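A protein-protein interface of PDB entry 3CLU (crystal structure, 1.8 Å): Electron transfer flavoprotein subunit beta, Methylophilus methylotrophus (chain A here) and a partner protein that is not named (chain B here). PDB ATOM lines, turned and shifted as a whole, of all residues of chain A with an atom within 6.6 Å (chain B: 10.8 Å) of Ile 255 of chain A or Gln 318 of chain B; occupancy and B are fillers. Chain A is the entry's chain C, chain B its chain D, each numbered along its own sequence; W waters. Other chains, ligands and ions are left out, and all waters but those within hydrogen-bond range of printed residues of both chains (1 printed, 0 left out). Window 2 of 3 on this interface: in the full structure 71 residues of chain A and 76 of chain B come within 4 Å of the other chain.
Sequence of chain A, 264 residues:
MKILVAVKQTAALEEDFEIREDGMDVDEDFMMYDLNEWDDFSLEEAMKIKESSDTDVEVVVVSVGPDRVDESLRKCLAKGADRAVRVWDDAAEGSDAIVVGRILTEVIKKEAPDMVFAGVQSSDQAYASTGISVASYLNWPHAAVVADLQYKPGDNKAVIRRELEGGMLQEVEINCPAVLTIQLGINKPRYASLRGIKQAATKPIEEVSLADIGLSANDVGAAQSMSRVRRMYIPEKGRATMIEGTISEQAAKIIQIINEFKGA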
ATOM      1  N   ILE A 247       7.041 -11.726 -15.462  1.00  0.00           N
ATOM      2  CA  ILE A 247       7.336 -11.150 -14.170  1.00  0.00           C
ATOM      3  C   ILE A 247       6.077 -10.569 -13.531  1.00  0.00           C
ATOM      4  O   ILE A 247       5.888 -10.733 -12.325  1.00  0.00           O
ATOM      5  CB  ILE A 247       8.445 -10.096 -14.315  1.00  0.00           C
ATOM      6  CG1 ILE A 247       9.772 -10.787 -14.670  1.00  0.00           C
ATOM      7  CG2 ILE A 247       8.541  -9.223 -13.074  1.00  0.00           C
ATOM      8  CD1 ILE A 247      10.453 -11.577 -13.517  1.00  0.00           C
ATOM      9  N   SER A 248       5.202  -9.946 -14.336  1.00  0.00           N
ATOM     10  CA  SER A 248       3.925  -9.367 -13.855  1.00  0.00           C
ATOM     11  C   SER A 248       3.021 -10.405 -13.210  1.00  0.00           C
ATOM     12  O   SER A 248       2.477 -10.202 -12.130  1.00  0.00           O
ATOM     13  CB  SER A 248       3.143  -8.689 -15.005  1.00  0.00           C
ATOM     14  N   GLU A 249       2.838 -11.516 -13.894  1.00  0.00           N
ATOM     15  CA  GLU A 249       1.964 -12.552 -13.369  1.00  0.00           C
ATOM     16  C   GLU A 249       2.568 -13.329 -12.231  1.00  0.00           C
ATOM     17  O   GLU A 249       1.833 -13.748 -11.350  1.00  0.00           O
ATOM     18  CB  GLU A 249       1.441 -13.497 -14.435  1.00  0.00           C
ATOM     19  CG  GLU A 249       2.420 -13.900 -15.482  1.00  0.00           C
ATOM     20  CD  GLU A 249       1.750 -14.113 -16.827  1.00  0.00           C
ATOM     21  OE1 GLU A 249       0.840 -13.341 -17.205  1.00  0.00           O
ATOM     22  OE2 GLU A 249       2.165 -15.051 -17.528  1.00  0.00           O
ATOM     23  N   GLN A 250       3.886 -13.528 -12.249  1.00  0.00           N
ATOM     24  CA  GLN A 250       4.575 -14.103 -11.100  1.00  0.00           C
ATOM     25  C   GLN A 250       4.359 -13.234  -9.872  1.00  0.00           C
ATOM     26  O   GLN A 250       3.976 -13.732  -8.814  1.00  0.00           O
ATOM     27  CB  GLN A 250       6.061 -14.323 -11.402  1.00  0.00           C
ATOM     28  CG  GLN A 250       6.284 -15.512 -12.345  1.00  0.00           C
ATOM     29  CD  GLN A 250       7.648 -15.546 -13.013  1.00  0.00           C
ATOM     30  OE1 GLN A 250       8.340 -14.533 -13.130  1.00  0.00           O
ATOM     31  NE2 GLN A 250       8.049 -16.736 -13.448  1.00  0.00           N
ATOM     32  N   ALA A 251       4.570 -11.929 -10.014  1.00  0.00           N
ATOM     33  CA  ALA A 251       4.333 -10.999  -8.912  1.00  0.00           C
ATOM     34  C   ALA A 251       2.856 -10.981  -8.495  1.00  0.00           C
ATOM     35  O   ALA A 251       2.530 -10.970  -7.307  1.00  0.00           O
ATOM     36  CB  ALA A 251       4.826  -9.602  -9.287  1.00  0.00           C
ATOM     37  N   ALA A 252       1.966 -11.003  -9.479  1.00  0.00           N
ATOM     38  CA  ALA A 252       0.546 -11.038  -9.215  1.00  0.00           C
ATOM     39  C   ALA A 252       0.203 -12.263  -8.339  1.00  0.00           C
ATOM     40  O   ALA A 252      -0.592 -12.161  -7.395  1.00  0.00           O
ATOM     41  CB  ALA A 252      -0.237 -11.065 -10.539  1.00  0.00           C
ATOM     42  N   LYS A 253       0.805 -13.411  -8.634  1.00  0.00           N
ATOM     43  CA  LYS A 253       0.491 -14.624  -7.882  1.00  0.00           C
ATOM     44  C   LYS A 253       1.030 -14.528  -6.453  1.00  0.00           C
ATOM     45  O   LYS A 253       0.342 -14.903  -5.508  1.00  0.00           O
ATOM     46  CB  LYS A 253       0.990 -15.876  -8.626  1.00  0.00           C
ATOM     47  CG  LYS A 253       0.769 -17.204  -7.918  1.00  0.00           C
ATOM     48  CD  LYS A 253      -0.673 -17.495  -7.650  1.00  0.00           C
ATOM     49  CE  LYS A 253      -0.806 -18.794  -6.937  1.00  0.00           C
ATOM     50  NZ  LYS A 253      -2.219 -19.143  -6.747  1.00  0.00           N
ATOM     51  N   ILE A 254       2.232 -13.973  -6.291  1.00  0.00           N
ATOM     52  CA  ILE A 254       2.794 -13.743  -4.950  1.00  0.00           C
ATOM     53  C   ILE A 254       1.868 -12.872  -4.114  1.00  0.00           C
ATOM     54  O   ILE A 254       1.627 -13.155  -2.947  1.00  0.00           O
ATOM     55  CB  ILE A 254       4.195 -13.088  -4.988  1.00  0.00           C
ATOM     56  CG1 ILE A 254       5.226 -14.066  -5.552  1.00  0.00           C
ATOM     57  CG2 ILE A 254       4.615 -12.656  -3.580  1.00  0.00           C
ATOM     58  CD1 ILE A 254       6.496 -13.432  -5.935  1.00  0.00           C
ATOM     59  N   ILE A 255       1.328 -11.825  -4.712  1.00  0.00           N
ATOM     60  CA  ILE A 255       0.473 -10.912  -3.970  1.00  0.00           C
ATOM     61  C   ILE A 255      -0.843 -11.599  -3.582  1.00  0.00           C
ATOM     62  O   ILE A 255      -1.399 -11.361  -2.512  1.00  0.00           O
ATOM     63  CB  ILE A 255       0.253  -9.622  -4.760  1.00  0.00           C
ATOM     64  CG1 ILE A 255       1.488  -8.733  -4.588  1.00  0.00           C
ATOM     65  CG2 ILE A 255      -1.012  -8.906  -4.293  1.00  0.00           C
ATOM     66  CD1 ILE A 255       1.538  -7.552  -5.502  1.00  0.00           C
ATOM     67  N   GLN A 256      -1.329 -12.469  -4.446  1.00  0.00           N
ATOM     68  CA  GLN A 256      -2.529 -13.235  -4.121  1.00  0.00           C
ATOM     69  C   GLN A 256      -2.303 -14.172  -2.950  1.00  0.00           C
ATOM     70  O   GLN A 256      -3.184 -14.363  -2.119  1.00  0.00           O
ATOM     71  CB  GLN A 256      -2.934 -14.053  -5.312  1.00  0.00           C
ATOM     72  CG  GLN A 256      -3.500 -13.214  -6.405  1.00  0.00           C
ATOM     73  CD  GLN A 256      -4.553 -13.941  -7.141  1.00  0.00           C
ATOM     74  OE1 GLN A 256      -4.602 -15.173  -7.080  1.00  0.00           O
ATOM     75  NE2 GLN A 256      -5.425 -13.207  -7.832  1.00  0.00           N
ATOM     76  N   ILE A 257      -1.104 -14.754  -2.897  1.00  0.00           N
ATOM     77  CA  ILE A 257      -0.701 -15.607  -1.795  1.00  0.00           C
ATOM     78  C   ILE A 257      -0.544 -14.758  -0.543  1.00  0.00           C
ATOM     79  O   ILE A 257      -0.933 -15.172   0.546  1.00  0.00           O
ATOM     80  CB  ILE A 257       0.600 -16.376  -2.119  1.00  0.00           C
ATOM     81  CG1 ILE A 257       0.375 -17.309  -3.315  1.00  0.00           C
ATOM     82  CG2 ILE A 257       1.080 -17.190  -0.920  1.00  0.00           C
ATOM     83  CD1 ILE A 257       1.677 -17.686  -4.011  1.00  0.00           C
ATOM     84  N   ILE A 258       0.014 -13.559  -0.689  1.00  0.00           N
ATOM     85  CA  ILE A 258       0.144 -12.651   0.452  1.00  0.00           C
ATOM     86  C   ILE A 258      -1.219 -12.238   0.986  1.00  0.00           C
ATOM     87  O   ILE A 258      -1.414 -12.102   2.198  1.00  0.00           O
ATOM     88  CB  ILE A 258       0.958 -11.381   0.095  1.00  0.00           C
ATOM     89  CG1 ILE A 258       2.425 -11.741  -0.118  1.00  0.00           C
ATOM     90  CG2 ILE A 258       0.803 -10.330   1.186  1.00  0.00           C
ATOM     91  CD1 ILE A 258       3.227 -10.622  -0.771  1.00  0.00           C
ATOM     92  N   ASN A 259      -2.160 -12.003   0.078  1.00  0.00           N
ATOM     93  CA  ASN A 259      -3.496 -11.623   0.480  1.00  0.00           C
ATOM     94  C   ASN A 259      -4.236 -12.790   1.113  1.00  0.00           C
ATOM     95  O   ASN A 259      -5.001 -12.589   2.055  1.00  0.00           O
ATOM     96  CB  ASN A 259      -4.282 -11.052  -0.707  1.00  0.00           C
ATOM     97  CG  ASN A 259      -3.734  -9.720  -1.183  1.00  0.00           C
ATOM     98  OD1 ASN A 259      -3.057  -9.005  -0.440  1.00  0.00           O
ATOM     99  ND2 ASN A 259      -4.013  -9.385  -2.437  1.00  0.00           N
ATOM    100  N   GLU A 260      -3.998 -14.005   0.610  1.00  0.00           N
ATOM    101  CA  GLU A 260      -4.594 -15.205   1.196  1.00  0.00           C
ATOM    102  C   GLU A 260      -4.117 -15.301   2.644  1.00  0.00           C
ATOM    103  O   GLU A 260      -4.910 -15.478   3.575  1.00  0.00           O
ATOM    104  CB  GLU A 260      -4.205 -16.459   0.409  1.00  0.00           C
ATOM    105  N   PHE B 205       5.132 -12.920   9.155  1.00  0.00           N
ATOM    106  CA  PHE B 205       5.327 -12.725   7.721  1.00  0.00           C
ATOM    107  C   PHE B 205       6.726 -12.174   7.470  1.00  0.00           C
ATOM    108  O   PHE B 205       7.065 -11.066   7.879  1.00  0.00           O
ATOM    109  CB  PHE B 205       4.225 -11.810   7.173  1.00  0.00           C
ATOM    110  CG  PHE B 205       4.355 -11.446   5.697  1.00  0.00           C
ATOM    111  CD1 PHE B 205       3.742 -10.288   5.215  1.00  0.00           C
ATOM    112  CD2 PHE B 205       5.033 -12.254   4.790  1.00  0.00           C
ATOM    113  CE1 PHE B 205       3.818  -9.942   3.869  1.00  0.00           C
ATOM    114  CE2 PHE B 205       5.108 -11.907   3.447  1.00  0.00           C
ATOM    115  CZ  PHE B 205       4.514 -10.765   2.990  1.00  0.00           C
ATOM    116  N   MET B 207       9.931 -11.558   4.606  1.00  0.00           N
ATOM    117  CA  MET B 207      10.694 -11.610   3.364  1.00  0.00           C
ATOM    118  C   MET B 207      12.184 -11.669   3.725  1.00  0.00           C
ATOM    119  O   MET B 207      12.691 -10.818   4.462  1.00  0.00           O
ATOM    120  CB  MET B 207      10.418 -10.398   2.510  1.00  0.00           C
ATOM    121  CG  MET B 207       8.999 -10.346   1.999  1.00  0.00           C
ATOM    122  SD  MET B 207       8.628  -8.804   1.203  1.00  0.00           S
ATOM    123  CE  MET B 207       7.135  -9.197   0.319  1.00  0.00           C
ATOM    124  N   LEU B 225      10.420  -3.007   0.031  1.00  0.00           N
ATOM    125  CA  LEU B 225       9.403  -3.983  -0.343  1.00  0.00           C
ATOM    126  C   LEU B 225       8.771  -4.602   0.907  1.00  0.00           C
ATOM    127  O   LEU B 225       7.537  -4.727   0.997  1.00  0.00           O
ATOM    128  CB  LEU B 225      10.010  -5.062  -1.229  1.00  0.00           C
ATOM    129  CG  LEU B 225       9.134  -6.274  -1.534  1.00  0.00           C
ATOM    130  CD1 LEU B 225       7.921  -5.862  -2.359  1.00  0.00           C
ATOM    131  CD2 LEU B 225       9.957  -7.357  -2.202  1.00  0.00           C
ATOM    132  N   GLU B 228       6.562  -2.050   2.476  1.00  0.00           N
ATOM    133  CA  GLU B 228       5.323  -1.929   1.689  1.00  0.00           C
ATOM    134  C   GLU B 228       4.373  -3.123   1.893  1.00  0.00           C
ATOM    135  O   GLU B 228       3.163  -2.933   2.046  1.00  0.00           O
ATOM    136  CB  GLU B 228       5.632  -1.750   0.198  1.00  0.00           C
ATOM    137  N   ALA B 229       4.923  -4.329   1.896  1.00  0.00           N
ATOM    138  CA  ALA B 229       4.153  -5.578   2.064  1.00  0.00           C
ATOM    139  C   ALA B 229       3.674  -5.819   3.500  1.00  0.00           C
ATOM    140  O   ALA B 229       2.719  -6.570   3.720  1.00  0.00           O
ATOM    141  CB  ALA B 229       4.991  -6.759   1.603  1.00  0.00           C
ATOM    142  N   GLY B 230       4.337  -5.185   4.467  1.00  0.00           N
ATOM    143  CA  GLY B 230       4.083  -5.432   5.881  1.00  0.00           C
ATOM    144  C   GLY B 230       4.789  -6.684   6.375  1.00  0.00           C
ATOM    145  O   GLY B 230       4.303  -7.370   7.274  1.00  0.00           O
ATOM    146  N   LEU B 263       4.195 -17.213   6.620  1.00  0.00           N
ATOM    147  CA  LEU B 263       4.529 -16.951   5.215  1.00  0.00           C
ATOM    148  C   LEU B 263       5.948 -16.426   5.158  1.00  0.00           C
ATOM    149  O   LEU B 263       6.260 -15.420   5.785  1.00  0.00           O
ATOM    150  CB  LEU B 263       3.564 -15.929   4.610  1.00  0.00           C
ATOM    151  CG  LEU B 263       3.822 -15.391   3.201  1.00  0.00           C
ATOM    152  CD1 LEU B 263       3.854 -16.495   2.154  1.00  0.00           C
ATOM    153  CD2 LEU B 263       2.762 -14.363   2.855  1.00  0.00           C
ATOM    154  N   VAL B 265       9.066 -15.565   2.424  1.00  0.00           N
ATOM    155  CA  VAL B 265       9.389 -15.373   1.017  1.00  0.00           C
ATOM    156  C   VAL B 265      10.896 -15.332   0.932  1.00  0.00           C
ATOM    157  O   VAL B 265      11.513 -14.387   1.415  1.00  0.00           O
ATOM    158  CB  VAL B 265       8.798 -14.100   0.455  1.00  0.00           C
ATOM    159  CG1 VAL B 265       9.084 -14.023  -1.028  1.00  0.00           C
ATOM    160  CG2 VAL B 265       7.294 -14.016   0.716  1.00  0.00           C
ATOM    161  N   THR B 284       3.690 -21.766   4.576  1.00  0.00           N
ATOM    162  CA  THR B 284       3.713 -21.286   3.201  1.00  0.00           C
ATOM    163  C   THR B 284       5.033 -20.601   2.938  1.00  0.00           C
ATOM    164  O   THR B 284       5.269 -19.512   3.415  1.00  0.00           O
ATOM    165  CB  THR B 284       2.538 -20.344   2.906  1.00  0.00           C
ATOM    166  OG1 THR B 284       1.310 -21.016   3.204  1.00  0.00           O
ATOM    167  CG2 THR B 284       2.523 -19.906   1.441  1.00  0.00           C
ATOM    168  N   ILE B 286       7.470 -19.273  -0.156  1.00  0.00           N
ATOM    169  CA  ILE B 286       7.630 -18.914  -1.559  1.00  0.00           C
ATOM    170  C   ILE B 286       9.126 -18.727  -1.768  1.00  0.00           C
ATOM    171  O   ILE B 286       9.787 -18.024  -1.003  1.00  0.00           O
ATOM    172  CB  ILE B 286       6.906 -17.596  -1.917  1.00  0.00           C
ATOM    173  CG1 ILE B 286       5.429 -17.643  -1.521  1.00  0.00           C
ATOM    174  CG2 ILE B 286       7.061 -17.282  -3.410  1.00  0.00           C
ATOM    175  CD1 ILE B 286       4.753 -16.308  -1.527  1.00  0.00           C
ATOM    176  N   VAL B 288      12.068 -17.443  -4.493  1.00  0.00           N
ATOM    177  CA  VAL B 288      12.377 -16.703  -5.714  1.00  0.00           C
ATOM    178  C   VAL B 288      13.863 -16.842  -5.971  1.00  0.00           C
ATOM    179  O   VAL B 288      14.673 -16.328  -5.228  1.00  0.00           O
ATOM    180  CB  VAL B 288      12.025 -15.188  -5.626  1.00  0.00           C
ATOM    181  CG1 VAL B 288      12.138 -14.541  -7.003  1.00  0.00           C
ATOM    182  CG2 VAL B 288      10.628 -14.967  -5.066  1.00  0.00           C
ATOM    183  N   TYR B 302       5.559 -22.670  -3.215  1.00  0.00           N
ATOM    184  CA  TYR B 302       5.563 -21.918  -4.454  1.00  0.00           C
ATOM    185  C   TYR B 302       6.979 -21.548  -4.872  1.00  0.00           C
ATOM    186  O   TYR B 302       7.777 -21.081  -4.073  1.00  0.00           O
ATOM    187  CB  TYR B 302       4.751 -20.630  -4.277  1.00  0.00           C
ATOM    188  CG  TYR B 302       3.310 -20.880  -3.900  1.00  0.00           C
ATOM    189  CD1 TYR B 302       2.888 -20.752  -2.587  1.00  0.00           C
ATOM    190  CD2 TYR B 302       2.392 -21.308  -4.839  1.00  0.00           C
ATOM    191  CE1 TYR B 302       1.575 -20.990  -2.225  1.00  0.00           C
ATOM    192  CE2 TYR B 302       1.069 -21.539  -4.495  1.00  0.00           C
ATOM    193  CZ  TYR B 302       0.674 -21.397  -3.179  1.00  0.00           C
ATOM    194  OH  TYR B 302      -0.622 -21.623  -2.826  1.00  0.00           O
ATOM    195  N   ILE B 304       9.244 -19.449  -7.840  1.00  0.00           N
ATOM    196  CA  ILE B 304       9.366 -18.573  -8.984  1.00  0.00           C
ATOM    197  C   ILE B 304      10.811 -18.549  -9.444  1.00  0.00           C
ATOM    198  O   ILE B 304      11.695 -18.071  -8.739  1.00  0.00           O
ATOM    199  CB  ILE B 304       8.882 -17.123  -8.686  1.00  0.00           C
ATOM    200  CG1 ILE B 304       7.350 -17.091  -8.629  1.00  0.00           C
ATOM    201  CG2 ILE B 304       9.369 -16.158  -9.787  1.00  0.00           C
ATOM    202  CD1 ILE B 304       6.808 -17.256  -7.228  1.00  0.00           C
ATOM    203  N   PHE B 309      15.375  -9.008  -8.461  1.00  0.00           N
ATOM    204  CA  PHE B 309      15.244  -7.550  -8.597  1.00  0.00           C
ATOM    205  C   PHE B 309      14.042  -7.217  -9.469  1.00  0.00           C
ATOM    206  O   PHE B 309      13.251  -6.335  -9.124  1.00  0.00           O
ATOM    207  CB  PHE B 309      16.522  -6.932  -9.154  1.00  0.00           C
ATOM    208  CG  PHE B 309      17.761  -7.411  -8.450  1.00  0.00           C
ATOM    209  CD1 PHE B 309      18.592  -8.357  -9.041  1.00  0.00           C
ATOM    210  CD2 PHE B 309      18.054  -6.971  -7.177  1.00  0.00           C
ATOM    211  CE1 PHE B 309      19.718  -8.817  -8.392  1.00  0.00           C
ATOM    212  CE2 PHE B 309      19.151  -7.431  -6.513  1.00  0.00           C
ATOM    213  CZ  PHE B 309      20.004  -8.349  -7.118  1.00  0.00           C
ATOM    214  N   ASP B 310      13.873  -7.948 -10.569  1.00  0.00           N
ATOM    215  CA  ASP B 310      12.697  -7.728 -11.420  1.00  0.00           C
ATOM    216  C   ASP B 310      11.398  -8.036 -10.661  1.00  0.00           C
ATOM    217  O   ASP B 310      10.415  -7.282 -10.750  1.00  0.00           O
ATOM    218  CB  ASP B 310      12.786  -8.570 -12.695  1.00  0.00           C
ATOM    219  CG  ASP B 310      13.907  -8.117 -13.609  1.00  0.00           C
ATOM    220  OD1 ASP B 310      14.415  -7.014 -13.411  1.00  0.00           O
ATOM    221  OD2 ASP B 310      14.273  -8.851 -14.543  1.00  0.00           O
ATOM    222  N   ILE B 311      11.401  -9.143  -9.924  1.00  0.00           N
ATOM    223  CA  ILE B 311      10.241  -9.541  -9.098  1.00  0.00           C
ATOM    224  C   ILE B 311       9.973  -8.470  -8.028  1.00  0.00           C
ATOM    225  O   ILE B 311       8.866  -7.979  -7.900  1.00  0.00           O
ATOM    226  CB  ILE B 311      10.470 -10.945  -8.464  1.00  0.00           C
ATOM    227  CG1 ILE B 311      10.407 -12.043  -9.543  1.00  0.00           C
ATOM    228  CG2 ILE B 311       9.465 -11.262  -7.342  1.00  0.00           C
ATOM    229  CD1 ILE B 311       8.993 -12.321 -10.082  1.00  0.00           C
ATOM    230  N   GLU B 312      11.001  -8.095  -7.281  1.00  0.00           N
ATOM    231  CA  GLU B 312      10.882  -7.037  -6.273  1.00  0.00           C
ATOM    232  C   GLU B 312      10.286  -5.720  -6.832  1.00  0.00           C
ATOM    233  O   GLU B 312       9.418  -5.127  -6.205  1.00  0.00           O
ATOM    234  CB  GLU B 312      12.250  -6.810  -5.605  1.00  0.00           C
ATOM    235  CG  GLU B 312      12.290  -5.656  -4.619  1.00  0.00           C
ATOM    236  CD  GLU B 312      12.569  -4.309  -5.279  1.00  0.00           C
ATOM    237  OE1 GLU B 312      13.465  -4.225  -6.156  1.00  0.00           O
ATOM    238  OE2 GLU B 312      11.908  -3.322  -4.900  1.00  0.00           O
ATOM    239  N   GLU B 313      10.768  -5.256  -7.989  1.00  0.00           N
ATOM    240  CA  GLU B 313      10.267  -4.002  -8.581  1.00  0.00           C
ATOM    241  C   GLU B 313       8.788  -4.099  -8.923  1.00  0.00           C
ATOM    242  O   GLU B 313       8.005  -3.189  -8.634  1.00  0.00           O
ATOM    243  CB  GLU B 313      11.058  -3.630  -9.841  1.00  0.00           C
ATOM    244  CG  GLU B 313      12.512  -3.273  -9.577  1.00  0.00           C
ATOM    245  CD  GLU B 313      13.349  -3.209 -10.859  1.00  0.00           C
ATOM    246  OE1 GLU B 313      12.767  -3.332 -11.970  1.00  0.00           O
ATOM    247  OE2 GLU B 313      14.587  -3.028 -10.746  1.00  0.00           O
ATOM    248  N   GLU B 314       8.412  -5.230  -9.514  1.00  0.00           N
ATOM    249  CA  GLU B 314       7.034  -5.467  -9.942  1.00  0.00           C
ATOM    250  C   GLU B 314       6.091  -5.655  -8.753  1.00  0.00           C
ATOM    251  O   GLU B 314       4.970  -5.155  -8.762  1.00  0.00           O
ATOM    252  CB  GLU B 314       6.995  -6.685 -10.852  1.00  0.00           C
ATOM    253  CG  GLU B 314       5.646  -6.970 -11.506  1.00  0.00           C
ATOM    254  CD  GLU B 314       5.148  -5.837 -12.385  1.00  0.00           C
ATOM    255  OE1 GLU B 314       5.971  -5.067 -12.945  1.00  0.00           O
ATOM    256  OE2 GLU B 314       3.917  -5.702 -12.518  1.00  0.00           O
ATOM    257  N   LEU B 315       6.536  -6.384  -7.737  1.00  0.00           N
ATOM    258  CA  LEU B 315       5.801  -6.468  -6.460  1.00  0.00           C
ATOM    259  C   LEU B 315       5.542  -5.085  -5.870  1.00  0.00           C
ATOM    260  O   LEU B 315       4.418  -4.769  -5.446  1.00  0.00           O
ATOM    261  CB  LEU B 315       6.609  -7.248  -5.430  1.00  0.00           C
ATOM    262  CG  LEU B 315       6.231  -8.595  -4.840  1.00  0.00           C
ATOM    263  CD1 LEU B 315       5.122  -9.395  -5.566  1.00  0.00           C
ATOM    264  CD2 LEU B 315       7.499  -9.399  -4.664  1.00  0.00           C
ATOM    265  N   LYS B 316       6.604  -4.282  -5.820  1.00  0.00           N
ATOM    266  CA  LYS B 316       6.532  -2.923  -5.306  1.00  0.00           C
ATOM    267  C   LYS B 316       5.504  -2.121  -6.066  1.00  0.00           C
ATOM    268  O   LYS B 316       4.700  -1.412  -5.458  1.00  0.00           O
ATOM    269  CB  LYS B 316       7.890  -2.217  -5.408  1.00  0.00           C
ATOM    270  N   ALA B 317       5.553  -2.220  -7.390  1.00  0.00           N
ATOM    271  CA  ALA B 317       4.649  -1.480  -8.247  1.00  0.00           C
ATOM    272  C   ALA B 317       3.216  -1.917  -7.991  1.00  0.00           C
ATOM    273  O   ALA B 317       2.326  -1.092  -7.778  1.00  0.00           O
ATOM    274  CB  ALA B 317       5.021  -1.685  -9.706  1.00  0.00           C
ATOM    275  N   GLN B 318       3.006  -3.226  -7.988  1.00  0.00           N
ATOM    276  CA  GLN B 318       1.672  -3.788  -7.820  1.00  0.00           C
ATOM    277  C   GLN B 318       1.076  -3.509  -6.443  1.00  0.00           C
ATOM    278  O   GLN B 318      -0.114  -3.241  -6.332  1.00  0.00           O
ATOM    279  CB  GLN B 318       1.685  -5.285  -8.101  1.00  0.00           C
ATOM    280  CG  GLN B 318       1.845  -5.607  -9.578  1.00  0.00           C
ATOM    281  CD  GLN B 318       1.668  -7.081  -9.897  1.00  0.00           C
ATOM    282  OE1 GLN B 318       1.025  -7.819  -9.147  1.00  0.00           O
ATOM    283  NE2 GLN B 318       2.214  -7.511 -11.030  1.00  0.00           N
ATOM    284  N   LEU B 319       1.895  -3.554  -5.398  1.00  0.00           N
ATOM    285  CA  LEU B 319       1.411  -3.273  -4.050  1.00  0.00           C
ATOM    286  C   LEU B 319       0.976  -1.802  -3.901  1.00  0.00           C
ATOM    287  O   LEU B 319      -0.035  -1.518  -3.267  1.00  0.00           O
ATOM    288  CB  LEU B 319       2.465  -3.645  -2.995  1.00  0.00           C
ATOM    289  CG  LEU B 319       2.718  -5.131  -2.741  1.00  0.00           C
ATOM    290  CD1 LEU B 319       3.996  -5.301  -1.956  1.00  0.00           C
ATOM    291  CD2 LEU B 319       1.553  -5.807  -2.004  1.00  0.00           C
ATOM    292  N   ALA B 320       1.718  -0.882  -4.517  1.00  0.00           N
ATOM    293  CA  ALA B 320       1.488   0.560  -4.359  1.00  0.00           C
ATOM    294  C   ALA B 320       0.207   1.039  -5.035  1.00  0.00           C
ATOM    295  O   ALA B 320      -0.149   0.572  -6.122  1.00  0.00           O
ATOM    296  CB  ALA B 320       2.688   1.345  -4.896  1.00  0.00           C
HETATM  297  O   HOH W   1      -2.901 -22.088  -5.178  1.00  0.00           O
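O of Ser 248 of chain A is in hydrogen-bond range of NE2 of Gln 318 of chain B, 2.9 Å away.
OE1 of Gln 318 of chain B sits close to N of Ala 252 of chain A (3.3 Å).
The backbone carbonyl oxygen of Ile 255 of chain A sits close to the side-chain amide nitrogen of Asn 259 of chain A, at 3.3 Å.
NE2 of Gln 318 of chain B lies within hydrogen-bond range of OE2 of Glu 314 of chain B (2.9 Å).
Among the printed residues, pairs that only touch across the chains: Ile 247 of chain A with Asp 310 of chain B, Ile 247 of chain A with Ile 311 of chain B, Ile 247 of chain A with Glu 314 of chain B, Ser 248 of chain A with Glu 314 of chain B, Gln 250 of chain A with Ile 304 of chain B, Gln 250 of chain A with Ile 311 of chain B, Ala 251 of chain A with Glu 314 of chain B, Ala 251 of chain A with Leu 315 of chain B, Ala 251 of chain A with Gln 318 of chain B, Ile 254 of chain A with Ile 304 of chain B, Ile 254 of chain A with Ile 311 of chain B, Ile 254 of chain A with Leu 315 of chain B, Ile 255 of chain A with Leu 315 of chain B, Ile 255 of chain A with Gln 318 of chain B, Ile 255 of chain A with Leu 319 of chain B, Ile 257 of chain A with Thr 284 of chain B, Ile 257 of chain A with Ile 286 of chain B, Ile 257 of chain A with Tyr 302 of chain B, Ile 258 of chain A with Phe 205 of chain B and Ile 258 of chain A with Leu 263 of chain B.
Of the printed residues of chain B, Ile 255 of chain A touches Leu 315 (3.8 Å), Gln 318 (3.5 Å) and Leu 319 (3.9 Å).
Of chain A, only Ser 248 (2.9 Å), Ala 251 (3.7 Å), Ala 252 (3.3 Å) and Ile 255 (3.5 Å) come within 4 Å of Gln 318 of chain B.
Ser 248 of chain A touches two residues of chain B.
Of the printed residues of chain B, Ala 252 of chain A touches Gln 318 (3.3 Å).
No residue of chain B comes within 4 Å of Gln 256 of chain A.
Of the printed residues of chain B, Ile 257 of chain A touches Thr 284 (3.9 Å), Ile 286 (3.8 Å) and Tyr 302 (3.6 Å).
Of the printed residues of chain B, Ile 258 of chain A touches Phe 205 and Leu 263.
Printed residues of chain A within 4 Å of Glu 314 of chain B: Ile 247 (3.7 Å), Ser 248 (3.8 Å) and Ala 251 (3.5 Å).
Of the printed residues of chain A, Leu 315 of chain B touches Ala 251, Ile 254 and Ile 255.
Of the printed residues of chain B, Ile 247 of chain A touches Asp 310 (3.6 Å), Ile 311 (3.8 Å) and Glu 314 (3.7 Å).
Of the printed residues of chain A, Leu 263 of chain B touches Ile 258.
Met 207 of chain B touches none of the printed residues of chain A.
Lys 316 of chain B touches none of the printed residues of chain A.
The nearest residue of chain B that does not touch Ile 255 of chain A is Glu 314 of chain B (5.3 Å).
Printed residues of chain A that touch a printed residue of chain B: Ile 247, Ser 248, Gln 250, Ala 251, Ala 252, Ile 254, Ile 255, Ile 257 and Ile 258.
Of the 25 printed residues of chain B, 12 touch a printed residue of chain A.
Hydrophobic or aromatic side chains of chain B that line the printed part of chain A: Phe 205, Leu 263, Ile 286, Tyr 302, Ile 304, Ile 311, Leu 315 and Leu 319.
Among the printed residues, 22 pairs touch across the chains.
Among the printed residues, no Asp or Glu carboxylate lies within 4 Å of a Lys or Arg side-chain nitrogen of the other chain.
Water W1 bridges OH of Tyr 302 of chain B (3.3 Å) and NZ of Lys 253 of chain A (3.4 Å).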
